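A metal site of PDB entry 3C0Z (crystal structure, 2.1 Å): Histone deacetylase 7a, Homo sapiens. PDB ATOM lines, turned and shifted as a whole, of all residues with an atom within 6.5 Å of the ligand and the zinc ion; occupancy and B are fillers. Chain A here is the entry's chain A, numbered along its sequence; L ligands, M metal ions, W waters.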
ATOM      1  N   ASP A 146      -1.118   4.249 -19.916  1.00  0.00           N
ATOM      2  CA  ASP A 146      -0.725   5.473 -20.599  1.00  0.00           C
ATOM      3  C   ASP A 146      -0.972   6.688 -19.754  1.00  0.00           C
ATOM      4  O   ASP A 146      -0.299   7.712 -19.869  1.00  0.00           O
ATOM      5  CB  ASP A 146      -1.580   5.655 -21.878  1.00  0.00           C
ATOM      6  CG  ASP A 146      -1.521   4.450 -22.817  1.00  0.00           C
ATOM      7  OD1 ASP A 146      -0.403   4.065 -23.206  1.00  0.00           O
ATOM      8  OD2 ASP A 146      -2.611   3.913 -23.181  1.00  0.00           O
ATOM      9  N   PRO A 187      -4.820  16.638 -22.061  1.00  0.00           N
ATOM     10  CA  PRO A 187      -5.901  16.709 -23.050  1.00  0.00           C
ATOM     11  C   PRO A 187      -7.241  16.271 -22.494  1.00  0.00           C
ATOM     12  O   PRO A 187      -7.284  15.836 -21.342  1.00  0.00           O
ATOM     13  CB  PRO A 187      -5.397  15.799 -24.179  1.00  0.00           C
ATOM     14  CG  PRO A 187      -4.518  14.810 -23.484  1.00  0.00           C
ATOM     15  CD  PRO A 187      -3.854  15.564 -22.366  1.00  0.00           C
ATOM     16  N   HIS A 189     -10.386  15.040 -24.751  1.00  0.00           N
ATOM     17  CA  HIS A 189     -11.444  14.496 -25.606  1.00  0.00           C
ATOM     18  C   HIS A 189     -11.787  13.004 -25.479  1.00  0.00           C
ATOM     19  O   HIS A 189     -12.872  12.591 -25.853  1.00  0.00           O
ATOM     20  CB  HIS A 189     -11.288  14.980 -27.071  1.00  0.00           C
ATOM     21  CG  HIS A 189     -10.243  14.257 -27.858  1.00  0.00           C
ATOM     22  ND1 HIS A 189     -10.425  13.932 -29.167  1.00  0.00           N
ATOM     23  CD2 HIS A 189      -9.019  13.802 -27.512  1.00  0.00           C
ATOM     24  CE1 HIS A 189      -9.351  13.302 -29.615  1.00  0.00           C
ATOM     25  NE2 HIS A 189      -8.493  13.186 -28.623  1.00  0.00           N
ATOM     26  N   HIS A 190     -10.929  12.217 -24.805  1.00  0.00           N
ATOM     27  CA  HIS A 190     -11.243  10.835 -24.533  1.00  0.00           C
ATOM     28  C   HIS A 190     -11.968  10.602 -23.206  1.00  0.00           C
ATOM     29  O   HIS A 190     -12.486   9.514 -22.990  1.00  0.00           O
ATOM     30  CB  HIS A 190      -9.953   9.985 -24.521  1.00  0.00           C
ATOM     31  CG  HIS A 190      -9.225   9.991 -25.827  1.00  0.00           C
ATOM     32  ND1 HIS A 190      -9.836   9.596 -27.003  1.00  0.00           N
ATOM     33  CD2 HIS A 190      -7.952  10.327 -26.147  1.00  0.00           C
ATOM     34  CE1 HIS A 190      -8.950   9.688 -27.990  1.00  0.00           C
ATOM     35  NE2 HIS A 190      -7.812  10.122 -27.500  1.00  0.00           N
ATOM     36  N   GLY A 198      -6.683   7.524 -22.218  1.00  0.00           N
ATOM     37  CA  GLY A 198      -6.050   8.204 -23.310  1.00  0.00           C
ATOM     38  C   GLY A 198      -5.427   9.533 -23.002  1.00  0.00           C
ATOM     39  O   GLY A 198      -5.470  10.460 -23.815  1.00  0.00           O
ATOM     40  N   PHE A 199      -4.775   9.627 -21.825  1.00  0.00           N
ATOM     41  CA  PHE A 199      -4.114  10.858 -21.421  1.00  0.00           C
ATOM     42  C   PHE A 199      -5.039  11.936 -20.849  1.00  0.00           C
ATOM     43  O   PHE A 199      -4.530  12.950 -20.388  1.00  0.00           O
ATOM     44  CB  PHE A 199      -3.211  11.476 -22.507  1.00  0.00           C
ATOM     45  CG  PHE A 199      -2.189  10.526 -23.118  1.00  0.00           C
ATOM     46  CD1 PHE A 199      -1.632   9.480 -22.388  1.00  0.00           C
ATOM     47  CD2 PHE A 199      -1.741  10.732 -24.450  1.00  0.00           C
ATOM     48  CE1 PHE A 199      -0.658   8.595 -22.990  1.00  0.00           C
ATOM     49  CE2 PHE A 199      -0.736   9.874 -25.047  1.00  0.00           C
ATOM     50  CZ  PHE A 199      -0.227   8.808 -24.308  1.00  0.00           C
ATOM     51  N   CYS A 200      -6.355  11.653 -20.781  1.00  0.00           N
ATOM     52  CA  CYS A 200      -7.417  12.621 -20.465  1.00  0.00           C
ATOM     53  C   CYS A 200      -8.136  12.259 -19.200  1.00  0.00           C
ATOM     54  O   CYS A 200      -8.412  11.075 -18.938  1.00  0.00           O
ATOM     55  CB  CYS A 200      -8.476  12.681 -21.598  1.00  0.00           C
ATOM     56  SG  CYS A 200      -7.848  12.983 -23.288  1.00  0.00           S
ATOM     57  N   ASP A 227      -8.058  16.370 -34.052  1.00  0.00           N
ATOM     58  CA  ASP A 227      -7.143  15.419 -33.501  1.00  0.00           C
ATOM     59  C   ASP A 227      -7.278  14.061 -34.300  1.00  0.00           C
ATOM     60  O   ASP A 227      -8.365  13.682 -34.682  1.00  0.00           O
ATOM     61  CB  ASP A 227      -7.502  15.212 -32.035  1.00  0.00           C
ATOM     62  CG  ASP A 227      -6.482  14.385 -31.303  1.00  0.00           C
ATOM     63  OD1 ASP A 227      -6.483  13.161 -31.494  1.00  0.00           O
ATOM     64  OD2 ASP A 227      -5.680  14.936 -30.515  1.00  0.00           O
ATOM     65  N   VAL A 228      -6.171  13.362 -34.534  1.00  0.00           N
ATOM     66  CA  VAL A 228      -6.187  12.149 -35.341  1.00  0.00           C
ATOM     67  C   VAL A 228      -6.996  11.002 -34.681  1.00  0.00           C
ATOM     68  O   VAL A 228      -7.395  10.052 -35.371  1.00  0.00           O
ATOM     69  CB  VAL A 228      -4.745  11.701 -35.720  1.00  0.00           C
ATOM     70  CG1 VAL A 228      -4.083  10.847 -34.614  1.00  0.00           C
ATOM     71  CG2 VAL A 228      -4.753  10.946 -37.105  1.00  0.00           C
ATOM     72  N   HIS A 229      -7.249  11.105 -33.368  1.00  0.00           N
ATOM     73  CA  HIS A 229      -8.010  10.088 -32.628  1.00  0.00           C
ATOM     74  C   HIS A 229      -9.465  10.525 -32.575  1.00  0.00           C
ATOM     75  O   HIS A 229      -9.760  11.738 -32.508  1.00  0.00           O
ATOM     76  CB  HIS A 229      -7.471   9.895 -31.208  1.00  0.00           C
ATOM     77  CG  HIS A 229      -6.041   9.435 -31.181  1.00  0.00           C
ATOM     78  ND1 HIS A 229      -4.992  10.294 -30.897  1.00  0.00           N
ATOM     79  CD2 HIS A 229      -5.487   8.221 -31.446  1.00  0.00           C
ATOM     80  CE1 HIS A 229      -3.857   9.615 -31.014  1.00  0.00           C
ATOM     81  NE2 HIS A 229      -4.134   8.364 -31.349  1.00  0.00           N
ATOM     82  N   HIS A 230     -10.397   9.576 -32.631  1.00  0.00           N
ATOM     83  CA  HIS A 230     -11.783   9.905 -32.291  1.00  0.00           C
ATOM     84  C   HIS A 230     -11.925  10.407 -30.802  1.00  0.00           C
ATOM     85  O   HIS A 230     -11.369   9.812 -29.865  1.00  0.00           O
ATOM     86  CB  HIS A 230     -12.673   8.676 -32.526  1.00  0.00           C
ATOM     87  CG  HIS A 230     -14.130   8.880 -32.187  1.00  0.00           C
ATOM     88  ND1 HIS A 230     -14.927   9.824 -32.803  1.00  0.00           N
ATOM     89  CD2 HIS A 230     -14.934   8.224 -31.331  1.00  0.00           C
ATOM     90  CE1 HIS A 230     -16.173   9.735 -32.335  1.00  0.00           C
ATOM     91  NE2 HIS A 230     -16.198   8.759 -31.440  1.00  0.00           N
ATOM     92  N   PHE A 258      -6.621   3.581 -31.998  1.00  0.00           N
ATOM     93  CA  PHE A 258      -7.074   4.078 -30.722  1.00  0.00           C
ATOM     94  C   PHE A 258      -8.034   5.262 -30.950  1.00  0.00           C
ATOM     95  O   PHE A 258      -7.774   6.137 -31.747  1.00  0.00           O
ATOM     96  CB  PHE A 258      -5.893   4.426 -29.782  1.00  0.00           C
ATOM     97  CG  PHE A 258      -6.318   4.835 -28.411  1.00  0.00           C
ATOM     98  CD1 PHE A 258      -6.675   6.172 -28.161  1.00  0.00           C
ATOM     99  CD2 PHE A 258      -6.397   3.905 -27.386  1.00  0.00           C
ATOM    100  CE1 PHE A 258      -7.127   6.568 -26.881  1.00  0.00           C
ATOM    101  CE2 PHE A 258      -6.839   4.291 -26.103  1.00  0.00           C
ATOM    102  CZ  PHE A 258      -7.201   5.635 -25.847  1.00  0.00           C
ATOM    103  N   GLY A 319      -6.077  18.833 -31.774  1.00  0.00           N
ATOM    104  CA  GLY A 319      -4.960  17.946 -31.596  1.00  0.00           C
ATOM    105  C   GLY A 319      -4.138  18.166 -32.838  1.00  0.00           C
ATOM    106  O   GLY A 319      -4.702  18.515 -33.893  1.00  0.00           O
ATOM    107  N   PHE A 320      -2.820  17.951 -32.705  1.00  0.00           N
ATOM    108  CA  PHE A 320      -1.928  18.100 -33.845  1.00  0.00           C
ATOM    109  C   PHE A 320      -1.191  16.850 -34.215  1.00  0.00           C
ATOM    110  O   PHE A 320      -0.187  16.941 -34.909  1.00  0.00           O
ATOM    111  CB  PHE A 320      -0.973  19.303 -33.688  1.00  0.00           C
ATOM    112  CG  PHE A 320      -1.684  20.589 -33.658  1.00  0.00           C
ATOM    113  CD1 PHE A 320      -1.603  21.404 -32.555  1.00  0.00           C
ATOM    114  CD2 PHE A 320      -2.559  20.923 -34.705  1.00  0.00           C
ATOM    115  CE1 PHE A 320      -2.317  22.576 -32.526  1.00  0.00           C
ATOM    116  CE2 PHE A 320      -3.281  22.066 -34.696  1.00  0.00           C
ATOM    117  CZ  PHE A 320      -3.165  22.918 -33.598  1.00  0.00           C
ATOM    118  N   ASP A 321      -1.718  15.693 -33.797  1.00  0.00           N
ATOM    119  CA  ASP A 321      -1.124  14.409 -34.069  1.00  0.00           C
ATOM    120  C   ASP A 321      -1.376  13.810 -35.472  1.00  0.00           C
ATOM    121  O   ASP A 321      -0.829  12.760 -35.822  1.00  0.00           O
ATOM    122  CB  ASP A 321      -1.458  13.405 -32.956  1.00  0.00           C
ATOM    123  CG  ASP A 321      -2.921  13.488 -32.454  1.00  0.00           C
ATOM    124  OD1 ASP A 321      -3.754  14.239 -32.996  1.00  0.00           O
ATOM    125  OD2 ASP A 321      -3.217  12.742 -31.513  1.00  0.00           O
ATOM    126  N   PRO A 329       2.291   4.347 -35.164  1.00  0.00           N
ATOM    127  CA  PRO A 329       1.359   4.012 -34.084  1.00  0.00           C
ATOM    128  C   PRO A 329       0.742   5.252 -33.390  1.00  0.00           C
ATOM    129  O   PRO A 329      -0.274   5.135 -32.725  1.00  0.00           O
ATOM    130  CB  PRO A 329       2.254   3.238 -33.086  1.00  0.00           C
ATOM    131  CG  PRO A 329       3.612   3.860 -33.266  1.00  0.00           C
ATOM    132  CD  PRO A 329       3.700   4.102 -34.774  1.00  0.00           C
ATOM    133  N   LEU A 330       1.362   6.402 -33.578  1.00  0.00           N
ATOM    134  CA  LEU A 330       0.944   7.644 -32.955  1.00  0.00           C
ATOM    135  C   LEU A 330       0.109   8.569 -33.871  1.00  0.00           C
ATOM    136  O   LEU A 330      -0.222   9.707 -33.476  1.00  0.00           O
ATOM    137  CB  LEU A 330       2.200   8.413 -32.501  1.00  0.00           C
ATOM    138  CG  LEU A 330       3.030   7.752 -31.411  1.00  0.00           C
ATOM    139  CD1 LEU A 330       4.373   8.365 -31.434  1.00  0.00           C
ATOM    140  CD2 LEU A 330       2.369   7.876 -30.011  1.00  0.00           C
ATOM    141  N   GLU A 360      -5.377  19.399 -27.788  1.00  0.00           N
ATOM    142  CA  GLU A 360      -5.673  18.041 -27.428  1.00  0.00           C
ATOM    143  C   GLU A 360      -4.366  17.287 -27.559  1.00  0.00           C
ATOM    144  O   GLU A 360      -3.461  17.564 -26.795  1.00  0.00           O
ATOM    145  CB  GLU A 360      -6.785  17.470 -28.323  1.00  0.00           C
ATOM    146  CG  GLU A 360      -8.143  18.213 -28.128  1.00  0.00           C
ATOM    147  CD  GLU A 360      -8.896  17.793 -26.868  1.00  0.00           C
ATOM    148  OE1 GLU A 360     -10.050  18.286 -26.636  1.00  0.00           O
ATOM    149  OE2 GLU A 360      -8.378  16.931 -26.131  1.00  0.00           O
ATOM    150  N   GLY A 361      -4.276  16.384 -28.518  1.00  0.00           N
ATOM    151  CA  GLY A 361      -3.112  15.508 -28.667  1.00  0.00           C
ATOM    152  C   GLY A 361      -2.041  16.064 -29.594  1.00  0.00           C
ATOM    153  O   GLY A 361      -2.057  17.233 -29.973  1.00  0.00           O
ATOM    154  N   GLY A 362      -1.096  15.235 -29.989  1.00  0.00           N
ATOM    155  CA  GLY A 362      -0.025  15.749 -30.847  1.00  0.00           C
ATOM    156  C   GLY A 362       1.162  16.013 -29.937  1.00  0.00           C
ATOM    157  O   GLY A 362       1.032  16.772 -28.968  1.00  0.00           O
HETATM  158  O1  LIG L   1      -6.136  11.897 -28.866  1.00  0.00           O
HETATM  159  O2  LIG L   1      -3.081  11.427 -28.500  1.00  0.00           O
HETATM  160  N1  LIG L   1      -5.105  12.052 -27.984  1.00  0.00           N
HETATM  161  C1  LIG L   1      -4.118  11.170 -27.937  1.00  0.00           C
HETATM  162  C2  LIG L   1      -4.361   9.885 -27.161  1.00  0.00           C
HETATM  163  C3  LIG L   1      -3.315   8.818 -27.487  1.00  0.00           C
HETATM  164  C4  LIG L   1      -3.561   7.520 -26.714  1.00  0.00           C
HETATM  165  C5  LIG L   1      -2.740   6.389 -27.347  1.00  0.00           C
HETATM  166 ZN    ZN M   1      -4.929  12.276 -30.488  1.00  0.00          ZN
HETATM  167  O   HOH W   1      -0.792  12.480 -28.644  1.00  0.00           O
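O1 of the ligand sits close to NE2 of His 189 (2.7 Å). A ring nitrogen (NE2) of His 190 lies close to an oxygen (O1) of the ligand (2.8 Å).
The backbone NH of Val 228 sits at hydrogen-bond distance from the side-chain carboxylate of Asp 321, 3.0 Å away. A ring nitrogen (NE2) of His 190 sits at hydrogen-bond distance from a ring nitrogen (NE2) of His 189. The side-chain carboxylate (OD2) of Asp 227 sits at hydrogen-bond distance from the backbone NH (N) of Gly 361, at 2.8 Å. SG of Cys 200 lies within hydrogen-bond range of O of Gly 198, at 3.5 Å. The backbone NH (N) of His 190 sits at hydrogen-bond distance from the side-chain sulfur (SG) of Cys 200 (3.5 Å). OE2 of Glu 360 sits at hydrogen-bond distance from N of His 189 (3.1 Å). N of His 189 is in hydrogen-bond range of SG of Cys 200. O of His 230 sits close to ND1 of His 190.
Gly 198 touches the ligand. CE2 of Phe 199 touches C3 of the ligand, at 3.7 Å. CD1 of Phe 258 touches C4 of the ligand, at 3.7 Å. Hydrophobic or aromatic side chains within 4 Å of the ligand: His 189, His 190, Phe 199, His 229 and Phe 258. Eight residues have an atom within 4 Å of the ligand: His 189, His 190, Gly 198, Phe 199, Asp 227, His 229, Phe 258 and Asp 321. The nearest printed residue that does not touch the ligand is Gly 361 (4.05 Å).
The zinc ion is bound by ND1 of His 229, at 2.0 Å. The side-chain carboxylate (OD2) of Asp 321 binds the zinc ion (2.0 Å). OD1 of Asp 227 binds the zinc ion, at 2.1 Å. The zinc ion is bound by an oxygen (O1) of the ligand (2.1 Å). Slightly farther from the zinc ion lies OD2 of Asp 227 (2.8 Å). Slightly farther from the zinc ion lies O2 of the ligand (2.8 Å).
Water W1 bridges O2 of the ligand (2.5 Å) and N of Gly 362 (3.1 Å).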
